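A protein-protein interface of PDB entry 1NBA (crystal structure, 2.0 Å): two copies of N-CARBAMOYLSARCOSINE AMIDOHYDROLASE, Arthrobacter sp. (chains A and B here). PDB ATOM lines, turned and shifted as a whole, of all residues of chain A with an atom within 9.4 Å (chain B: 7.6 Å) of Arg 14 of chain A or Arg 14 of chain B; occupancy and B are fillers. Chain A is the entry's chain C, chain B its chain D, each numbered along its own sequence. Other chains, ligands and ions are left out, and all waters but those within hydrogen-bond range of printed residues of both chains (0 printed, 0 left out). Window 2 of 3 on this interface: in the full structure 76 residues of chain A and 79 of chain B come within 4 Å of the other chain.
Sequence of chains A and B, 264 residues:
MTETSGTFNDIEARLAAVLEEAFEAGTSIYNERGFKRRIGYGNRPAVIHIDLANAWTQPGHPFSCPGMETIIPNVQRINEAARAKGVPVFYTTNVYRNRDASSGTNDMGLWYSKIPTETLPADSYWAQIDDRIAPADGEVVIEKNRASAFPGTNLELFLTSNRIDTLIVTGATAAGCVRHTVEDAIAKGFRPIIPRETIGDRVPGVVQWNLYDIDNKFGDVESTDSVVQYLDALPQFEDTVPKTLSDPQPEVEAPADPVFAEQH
NH2 of Arg 14 of chain B lies within salt-bridge range of OE1 of Glu 21 of chain A (3.0 Å).
ND2 of Asn 9 of chain B lies close to NH2 of Arg 14 of chain B (3.0 Å).
Glu 21 of chain B touches Ile 11 of chain A. Arg 14 of chain A touches Arg 14 of chain B. CA of Leu 15 of chain A touches CG2 of Val 18 of chain B, 3.7 Å away. Val 18 of chain A touches Leu 15 of chain B (CG1 to CA, 3.7 Å). CG1 of Val 18 of chain A touches CG1 of Val 18 of chain B, at 3.4 Å. Ile 11 of chain B touches Glu 21 of chain A (CG1 to OE1, 3.8 Å). Ala 22 of chain A touches Leu 15 of chain B (CB to CD2, 3.7 Å).
No residue of chain B comes within 4 Å of Ala 13 of chain A. Of chain B, only Arg 14 (3.97 Å) comes within 4 Å of Arg 14 of chain A. Printed residues of chain B within 4 Å of Leu 15 of chain A: Val 18 (3.7 Å). Printed residues of chain B within 4 Å of Val 18 of chain A: Leu 15 (3.7 Å) and Val 18 (3.4 Å). Of the printed residues of chain B, Ala 22 of chain A touches Leu 15. No residue of chain A comes within 4 Å of Asp 10 of chain B. Ala 13 of chain B touches none of the printed residues of chain A. Of the printed residues of chain A, Arg 14 of chain B touches Arg 14 (3.97 Å) and Glu 21 (3.0 Å). No residue of chain A comes within 4 Å of Ala 17 of chain B. Of the printed residues of chain A, Val 18 of chain B touches Leu 15 and Val 18. Of the printed residues of chain A, Glu 21 of chain B touches Ile 11.
Of the 14 printed residues of chain B, 5 touch a printed residue of chain A. Hydrophobic or aromatic side chains of chain B that line the printed part of chain A: Ile 11, Leu 15 and Val 18.
Ile 11 of chain A touches Glu 21 of chain B, and with the chains exchanged Glu 21 of chain A touches Ile 11 of chain B. Arg 14 of chain A touches its own counterpart, Arg 14 of chain B. Leu 15 of chain A touches Val 18 of chain B, and with the chains exchanged Val 18 of chain A touches Leu 15 of chain B. Glu 21 of chain A touches Arg 14 of chain B, but with the chains exchanged Arg 14 of chain A does not touch Glu 21 of chain B (5.5 Å).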
ATOM      1  N   ASN A   9      -0.987 -28.870   0.673  1.00  0.00           N
ATOM      2  CA  ASN A   9      -0.754 -29.569   1.940  1.00  0.00           C
ATOM      3  C   ASN A   9       0.696 -29.534   2.419  1.00  0.00           C
ATOM      4  O   ASN A   9       0.947 -29.468   3.629  1.00  0.00           O
ATOM      5  N   ASP A  10       1.663 -29.585   1.491  1.00  0.00           N
ATOM      6  CA  ASP A  10       3.084 -29.508   1.840  1.00  0.00           C
ATOM      7  C   ASP A  10       3.381 -28.193   2.561  1.00  0.00           C
ATOM      8  O   ASP A  10       4.133 -28.151   3.542  1.00  0.00           O
ATOM      9  N   ILE A  11       2.710 -27.135   2.086  1.00  0.00           N
ATOM     10  CA  ILE A  11       2.805 -25.830   2.704  1.00  0.00           C
ATOM     11  C   ILE A  11       2.124 -25.972   4.054  1.00  0.00           C
ATOM     12  O   ILE A  11       2.746 -25.537   5.008  1.00  0.00           O
ATOM     13  CB  ILE A  11       2.112 -24.749   1.809  1.00  0.00           C
ATOM     14  CG1 ILE A  11       3.038 -24.514   0.612  1.00  0.00           C
ATOM     15  CG2 ILE A  11       1.831 -23.442   2.564  1.00  0.00           C
ATOM     16  CD1 ILE A  11       2.489 -23.606  -0.511  1.00  0.00           C
ATOM     17  N   GLU A  12       0.946 -26.585   4.241  1.00  0.00           N
ATOM     18  CA  GLU A  12       0.315 -26.708   5.561  1.00  0.00           C
ATOM     19  C   GLU A  12       1.237 -27.288   6.640  1.00  0.00           C
ATOM     20  O   GLU A  12       1.338 -26.748   7.748  1.00  0.00           O
ATOM     21  CB  GLU A  12      -0.952 -27.569   5.418  1.00  0.00           C
ATOM     22  N   ALA A  13       1.949 -28.361   6.308  1.00  0.00           N
ATOM     23  CA  ALA A  13       2.881 -28.980   7.232  1.00  0.00           C
ATOM     24  C   ALA A  13       4.147 -28.150   7.408  1.00  0.00           C
ATOM     25  O   ALA A  13       4.594 -27.983   8.545  1.00  0.00           O
ATOM     26  CB  ALA A  13       3.271 -30.362   6.730  1.00  0.00           C
ATOM     27  N   ARG A  14       4.744 -27.606   6.336  1.00  0.00           N
ATOM     28  CA  ARG A  14       5.927 -26.743   6.418  1.00  0.00           C
ATOM     29  C   ARG A  14       5.578 -25.545   7.290  1.00  0.00           C
ATOM     30  O   ARG A  14       6.282 -25.203   8.232  1.00  0.00           O
ATOM     31  CB  ARG A  14       6.339 -26.197   5.045  1.00  0.00           C
ATOM     32  CG  ARG A  14       7.792 -26.368   4.636  1.00  0.00           C
ATOM     33  CD  ARG A  14       8.836 -25.506   5.337  1.00  0.00           C
ATOM     34  NE  ARG A  14       9.759 -26.309   6.129  1.00  0.00           N
ATOM     35  CZ  ARG A  14      11.095 -26.151   6.107  1.00  0.00           C
ATOM     36  NH1 ARG A  14      11.716 -25.250   5.352  1.00  0.00           N
ATOM     37  NH2 ARG A  14      11.836 -26.920   6.899  1.00  0.00           N
ATOM     38  N   LEU A  15       4.429 -24.952   6.996  1.00  0.00           N
ATOM     39  CA  LEU A  15       3.908 -23.782   7.668  1.00  0.00           C
ATOM     40  C   LEU A  15       3.774 -24.118   9.127  1.00  0.00           C
ATOM     41  O   LEU A  15       4.367 -23.393   9.921  1.00  0.00           O
ATOM     42  CB  LEU A  15       2.538 -23.366   7.109  1.00  0.00           C
ATOM     43  CG  LEU A  15       1.838 -22.149   7.710  1.00  0.00           C
ATOM     44  CD1 LEU A  15       2.673 -20.909   7.515  1.00  0.00           C
ATOM     45  CD2 LEU A  15       0.514 -21.930   7.023  1.00  0.00           C
ATOM     46  N   ALA A  16       3.113 -25.203   9.528  1.00  0.00           N
ATOM     47  CA  ALA A  16       2.985 -25.543  10.946  1.00  0.00           C
ATOM     48  C   ALA A  16       4.321 -25.670  11.672  1.00  0.00           C
ATOM     49  O   ALA A  16       4.525 -25.145  12.770  1.00  0.00           O
ATOM     50  CB  ALA A  16       2.249 -26.860  11.113  1.00  0.00           C
ATOM     51  N   ALA A  17       5.260 -26.327  11.005  1.00  0.00           N
ATOM     52  CA  ALA A  17       6.582 -26.505  11.575  1.00  0.00           C
ATOM     53  C   ALA A  17       7.360 -25.195  11.704  1.00  0.00           C
ATOM     54  O   ALA A  17       7.894 -24.910  12.775  1.00  0.00           O
ATOM     55  CB  ALA A  17       7.396 -27.460  10.710  1.00  0.00           C
ATOM     56  N   VAL A  18       7.406 -24.355  10.676  1.00  0.00           N
ATOM     57  CA  VAL A  18       8.158 -23.120  10.741  1.00  0.00           C
ATOM     58  C   VAL A  18       7.490 -22.145  11.715  1.00  0.00           C
ATOM     59  O   VAL A  18       8.184 -21.500  12.514  1.00  0.00           O
ATOM     60  CB  VAL A  18       8.271 -22.546   9.326  1.00  0.00           C
ATOM     61  CG1 VAL A  18       9.097 -21.277   9.337  1.00  0.00           C
ATOM     62  CG2 VAL A  18       9.039 -23.511   8.442  1.00  0.00           C
ATOM     63  N   LEU A  19       6.151 -22.045  11.725  1.00  0.00           N
ATOM     64  CA  LEU A  19       5.439 -21.230  12.708  1.00  0.00           C
ATOM     65  C   LEU A  19       5.810 -21.694  14.109  1.00  0.00           C
ATOM     66  O   LEU A  19       6.026 -20.842  14.967  1.00  0.00           O
ATOM     67  CB  LEU A  19       3.916 -21.339  12.585  1.00  0.00           C
ATOM     68  CG  LEU A  19       3.272 -20.641  11.398  1.00  0.00           C
ATOM     69  CD1 LEU A  19       1.812 -21.033  11.284  1.00  0.00           C
ATOM     70  CD2 LEU A  19       3.432 -19.132  11.580  1.00  0.00           C
ATOM     71  N   GLU A  20       5.953 -22.999  14.382  1.00  0.00           N
ATOM     72  CA  GLU A  20       6.367 -23.444  15.708  1.00  0.00           C
ATOM     73  C   GLU A  20       7.750 -22.908  16.068  1.00  0.00           C
ATOM     74  O   GLU A  20       7.957 -22.520  17.221  1.00  0.00           O
ATOM     75  CB  GLU A  20       6.386 -24.972  15.800  1.00  0.00           C
ATOM     76  CG  GLU A  20       6.682 -25.497  17.222  1.00  0.00           C
ATOM     77  CD  GLU A  20       5.767 -24.976  18.339  1.00  0.00           C
ATOM     78  N   GLU A  21       8.682 -22.844  15.111  1.00  0.00           N
ATOM     79  CA  GLU A  21       9.985 -22.246  15.350  1.00  0.00           C
ATOM     80  C   GLU A  21       9.776 -20.788  15.734  1.00  0.00           C
ATOM     81  O   GLU A  21      10.280 -20.353  16.769  1.00  0.00           O
ATOM     82  CB  GLU A  21      10.845 -22.209  14.142  1.00  0.00           C
ATOM     83  CG  GLU A  21      11.186 -23.518  13.493  1.00  0.00           C
ATOM     84  CD  GLU A  21      11.874 -23.305  12.148  1.00  0.00           C
ATOM     85  OE1 GLU A  21      12.700 -22.401  12.034  1.00  0.00           O
ATOM     86  OE2 GLU A  21      11.585 -24.039  11.202  1.00  0.00           O
ATOM     87  N   ALA A  22       9.006 -20.023  14.949  1.00  0.00           N
ATOM     88  CA  ALA A  22       8.737 -18.626  15.247  1.00  0.00           C
ATOM     89  C   ALA A  22       8.090 -18.423  16.603  1.00  0.00           C
ATOM     90  O   ALA A  22       8.428 -17.485  17.326  1.00  0.00           O
ATOM     91  CB  ALA A  22       7.818 -18.035  14.209  1.00  0.00           C
ATOM     92  N   ALA A  25      10.737 -19.146  19.489  1.00  0.00           N
ATOM     93  CA  ALA A  25      11.616 -18.000  19.579  1.00  0.00           C
ATOM     94  C   ALA A  25      10.911 -16.834  20.254  1.00  0.00           C
ATOM     95  O   ALA A  25      11.424 -16.242  21.208  1.00  0.00           O
ATOM     96  CB  ALA A  25      12.030 -17.568  18.199  1.00  0.00           C
ATOM     97  N   GLN A 208      -3.493 -20.429  14.140  1.00  0.00           N
ATOM     98  CA  GLN A 208      -2.264 -20.608  14.879  1.00  0.00           C
ATOM     99  C   GLN A 208      -1.676 -19.273  15.302  1.00  0.00           C
ATOM    100  O   GLN A 208      -1.552 -19.042  16.507  1.00  0.00           O
ATOM    101  CB  GLN A 208      -1.257 -21.358  14.030  1.00  0.00           C
ATOM    102  CG  GLN A 208      -1.625 -22.818  13.794  1.00  0.00           C
ATOM    103  CD  GLN A 208      -0.714 -23.471  12.767  1.00  0.00           C
ATOM    104  OE1 GLN A 208      -1.046 -23.598  11.575  1.00  0.00           O
ATOM    105  NE2 GLN A 208       0.469 -23.885  13.201  1.00  0.00           N
ATOM    106  N   PHE B   8      24.215 -19.678  13.717  1.00  0.00           N
ATOM    107  CA  PHE B   8      23.469 -18.826  12.802  1.00  0.00           C
ATOM    108  C   PHE B   8      22.399 -19.799  12.363  1.00  0.00           C
ATOM    109  O   PHE B   8      22.662 -20.952  12.017  1.00  0.00           O
ATOM    110  CB  PHE B   8      24.191 -18.377  11.505  1.00  0.00           C
ATOM    111  CG  PHE B   8      23.291 -17.548  10.580  1.00  0.00           C
ATOM    112  CD1 PHE B   8      22.860 -16.290  10.964  1.00  0.00           C
ATOM    113  CD2 PHE B   8      22.888 -18.060   9.357  1.00  0.00           C
ATOM    114  CE1 PHE B   8      22.033 -15.557  10.135  1.00  0.00           C
ATOM    115  CE2 PHE B   8      22.060 -17.319   8.537  1.00  0.00           C
ATOM    116  CZ  PHE B   8      21.632 -16.068   8.922  1.00  0.00           C
ATOM    117  N   ASN B   9      21.171 -19.326  12.422  1.00  0.00           N
ATOM    118  CA  ASN B   9      20.048 -20.117  11.983  1.00  0.00           C
ATOM    119  C   ASN B   9      19.298 -19.151  11.090  1.00  0.00           C
ATOM    120  O   ASN B   9      19.030 -18.007  11.487  1.00  0.00           O
ATOM    121  CB  ASN B   9      19.186 -20.535  13.161  1.00  0.00           C
ATOM    122  CG  ASN B   9      18.102 -21.509  12.729  1.00  0.00           C
ATOM    123  OD1 ASN B   9      18.251 -22.320  11.811  1.00  0.00           O
ATOM    124  ND2 ASN B   9      16.949 -21.469  13.371  1.00  0.00           N
ATOM    125  N   ASP B  10      18.966 -19.557   9.877  1.00  0.00           N
ATOM    126  CA  ASP B  10      18.312 -18.681   8.925  1.00  0.00           C
ATOM    127  C   ASP B  10      16.802 -18.529   9.131  1.00  0.00           C
ATOM    128  O   ASP B  10      16.042 -18.322   8.176  1.00  0.00           O
ATOM    129  CB  ASP B  10      18.675 -19.247   7.564  1.00  0.00           C
ATOM    130  CG  ASP B  10      18.516 -18.277   6.414  1.00  0.00           C
ATOM    131  OD1 ASP B  10      18.972 -17.135   6.506  1.00  0.00           O
ATOM    132  OD2 ASP B  10      17.930 -18.690   5.418  1.00  0.00           O
ATOM    133  N   ILE B  11      16.387 -18.483  10.406  1.00  0.00           N
ATOM    134  CA  ILE B  11      14.981 -18.482  10.780  1.00  0.00           C
ATOM    135  C   ILE B  11      14.175 -17.319  10.219  1.00  0.00           C
ATOM    136  O   ILE B  11      13.066 -17.560   9.744  1.00  0.00           O
ATOM    137  CB  ILE B  11      14.857 -18.538  12.345  1.00  0.00           C
ATOM    138  CG1 ILE B  11      13.380 -18.686  12.687  1.00  0.00           C
ATOM    139  CG2 ILE B  11      15.489 -17.322  13.022  1.00  0.00           C
ATOM    140  CD1 ILE B  11      13.083 -18.696  14.186  1.00  0.00           C
ATOM    141  N   GLU B  12      14.716 -16.099  10.195  1.00  0.00           N
ATOM    142  CA  GLU B  12      13.994 -14.948   9.676  1.00  0.00           C
ATOM    143  C   GLU B  12      13.673 -15.143   8.207  1.00  0.00           C
ATOM    144  O   GLU B  12      12.523 -15.018   7.789  1.00  0.00           O
ATOM    145  CB  GLU B  12      14.798 -13.664   9.789  1.00  0.00           C
ATOM    146  CG  GLU B  12      14.693 -12.832  11.060  1.00  0.00           C
ATOM    147  CD  GLU B  12      15.428 -13.352  12.293  1.00  0.00           C
ATOM    148  OE1 GLU B  12      16.663 -13.278  12.331  1.00  0.00           O
ATOM    149  OE2 GLU B  12      14.761 -13.807  13.229  1.00  0.00           O
ATOM    150  N   ALA B  13      14.668 -15.494   7.396  1.00  0.00           N
ATOM    151  CA  ALA B  13      14.451 -15.677   5.973  1.00  0.00           C
ATOM    152  C   ALA B  13      13.618 -16.921   5.688  1.00  0.00           C
ATOM    153  O   ALA B  13      12.808 -16.892   4.755  1.00  0.00           O
ATOM    154  CB  ALA B  13      15.772 -15.803   5.250  1.00  0.00           C
ATOM    155  N   ARG B  14      13.773 -18.008   6.438  1.00  0.00           N
ATOM    156  CA  ARG B  14      12.950 -19.194   6.265  1.00  0.00           C
ATOM    157  C   ARG B  14      11.477 -18.877   6.587  1.00  0.00           C
ATOM    158  O   ARG B  14      10.587 -19.182   5.789  1.00  0.00           O
ATOM    159  CB  ARG B  14      13.497 -20.281   7.168  1.00  0.00           C
ATOM    160  CG  ARG B  14      12.655 -21.552   7.232  1.00  0.00           C
ATOM    161  CD  ARG B  14      13.385 -22.703   7.895  1.00  0.00           C
ATOM    162  NE  ARG B  14      13.800 -22.420   9.250  1.00  0.00           N
ATOM    163  CZ  ARG B  14      15.081 -22.221   9.572  1.00  0.00           C
ATOM    164  NH1 ARG B  14      16.062 -22.257   8.667  1.00  0.00           N
ATOM    165  NH2 ARG B  14      15.392 -22.014  10.844  1.00  0.00           N
ATOM    166  N   LEU B  15      11.194 -18.225   7.720  1.00  0.00           N
ATOM    167  CA  LEU B  15       9.836 -17.849   8.104  1.00  0.00           C
ATOM    168  C   LEU B  15       9.252 -16.865   7.089  1.00  0.00           C
ATOM    169  O   LEU B  15       8.104 -17.028   6.686  1.00  0.00           O
ATOM    170  CB  LEU B  15       9.848 -17.233   9.503  1.00  0.00           C
ATOM    171  CG  LEU B  15       8.582 -16.687  10.161  1.00  0.00           C
ATOM    172  CD1 LEU B  15       7.578 -17.778  10.510  1.00  0.00           C
ATOM    173  CD2 LEU B  15       9.019 -15.994  11.427  1.00  0.00           C
ATOM    174  N   ALA B  16       9.997 -15.854   6.597  1.00  0.00           N
ATOM    175  CA  ALA B  16       9.454 -14.935   5.609  1.00  0.00           C
ATOM    176  C   ALA B  16       9.060 -15.653   4.322  1.00  0.00           C
ATOM    177  O   ALA B  16       7.992 -15.381   3.741  1.00  0.00           O
ATOM    178  CB  ALA B  16      10.477 -13.867   5.251  1.00  0.00           C
ATOM    179  N   ALA B  17       9.863 -16.609   3.880  1.00  0.00           N
ATOM    180  CA  ALA B  17       9.538 -17.363   2.682  1.00  0.00           C
ATOM    181  C   ALA B  17       8.296 -18.241   2.886  1.00  0.00           C
ATOM    182  O   ALA B  17       7.412 -18.241   2.018  1.00  0.00           O
ATOM    183  CB  ALA B  17      10.738 -18.237   2.306  1.00  0.00           C
ATOM    184  N   VAL B  18       8.115 -18.954   4.001  1.00  0.00           N
ATOM    185  CA  VAL B  18       6.906 -19.768   4.103  1.00  0.00           C
ATOM    186  C   VAL B  18       5.672 -18.932   4.457  1.00  0.00           C
ATOM    187  O   VAL B  18       4.567 -19.232   3.978  1.00  0.00           O
ATOM    188  CB  VAL B  18       7.159 -20.935   5.127  1.00  0.00           C
ATOM    189  CG1 VAL B  18       7.485 -20.385   6.473  1.00  0.00           C
ATOM    190  CG2 VAL B  18       5.910 -21.794   5.268  1.00  0.00           C
ATOM    191  N   LEU B  19       5.788 -17.856   5.245  1.00  0.00           N
ATOM    192  CA  LEU B  19       4.647 -16.977   5.496  1.00  0.00           C
ATOM    193  C   LEU B  19       4.201 -16.417   4.158  1.00  0.00           C
ATOM    194  O   LEU B  19       3.004 -16.391   3.900  1.00  0.00           O
ATOM    195  CB  LEU B  19       5.003 -15.787   6.395  1.00  0.00           C
ATOM    196  CG  LEU B  19       5.158 -16.038   7.871  1.00  0.00           C
ATOM    197  CD1 LEU B  19       5.513 -14.746   8.572  1.00  0.00           C
ATOM    198  CD2 LEU B  19       3.857 -16.589   8.430  1.00  0.00           C
ATOM    199  N   GLU B  20       5.109 -16.052   3.240  1.00  0.00           N
ATOM    200  CA  GLU B  20       4.696 -15.555   1.937  1.00  0.00           C
ATOM    201  C   GLU B  20       3.871 -16.622   1.214  1.00  0.00           C
ATOM    202  O   GLU B  20       2.827 -16.298   0.624  1.00  0.00           O
ATOM    203  CB  GLU B  20       5.901 -15.196   1.096  1.00  0.00           C
ATOM    204  CG  GLU B  20       5.466 -14.289  -0.044  1.00  0.00           C
ATOM    205  N   GLU B  21       4.253 -17.891   1.286  1.00  0.00           N
ATOM    206  CA  GLU B  21       3.463 -18.965   0.709  1.00  0.00           C
ATOM    207  C   GLU B  21       2.089 -19.012   1.349  1.00  0.00           C
ATOM    208  O   GLU B  21       1.102 -19.173   0.628  1.00  0.00           O
ATOM    209  CB  GLU B  21       4.104 -20.308   0.906  1.00  0.00           C
ATOM    210  CG  GLU B  21       5.453 -20.367   0.212  1.00  0.00           C
ATOM    211  CD  GLU B  21       6.113 -21.734   0.311  1.00  0.00           C
ATOM    212  OE1 GLU B  21       6.538 -22.124   1.401  1.00  0.00           O
ATOM    213  OE2 GLU B  21       6.187 -22.405  -0.716  1.00  0.00           O
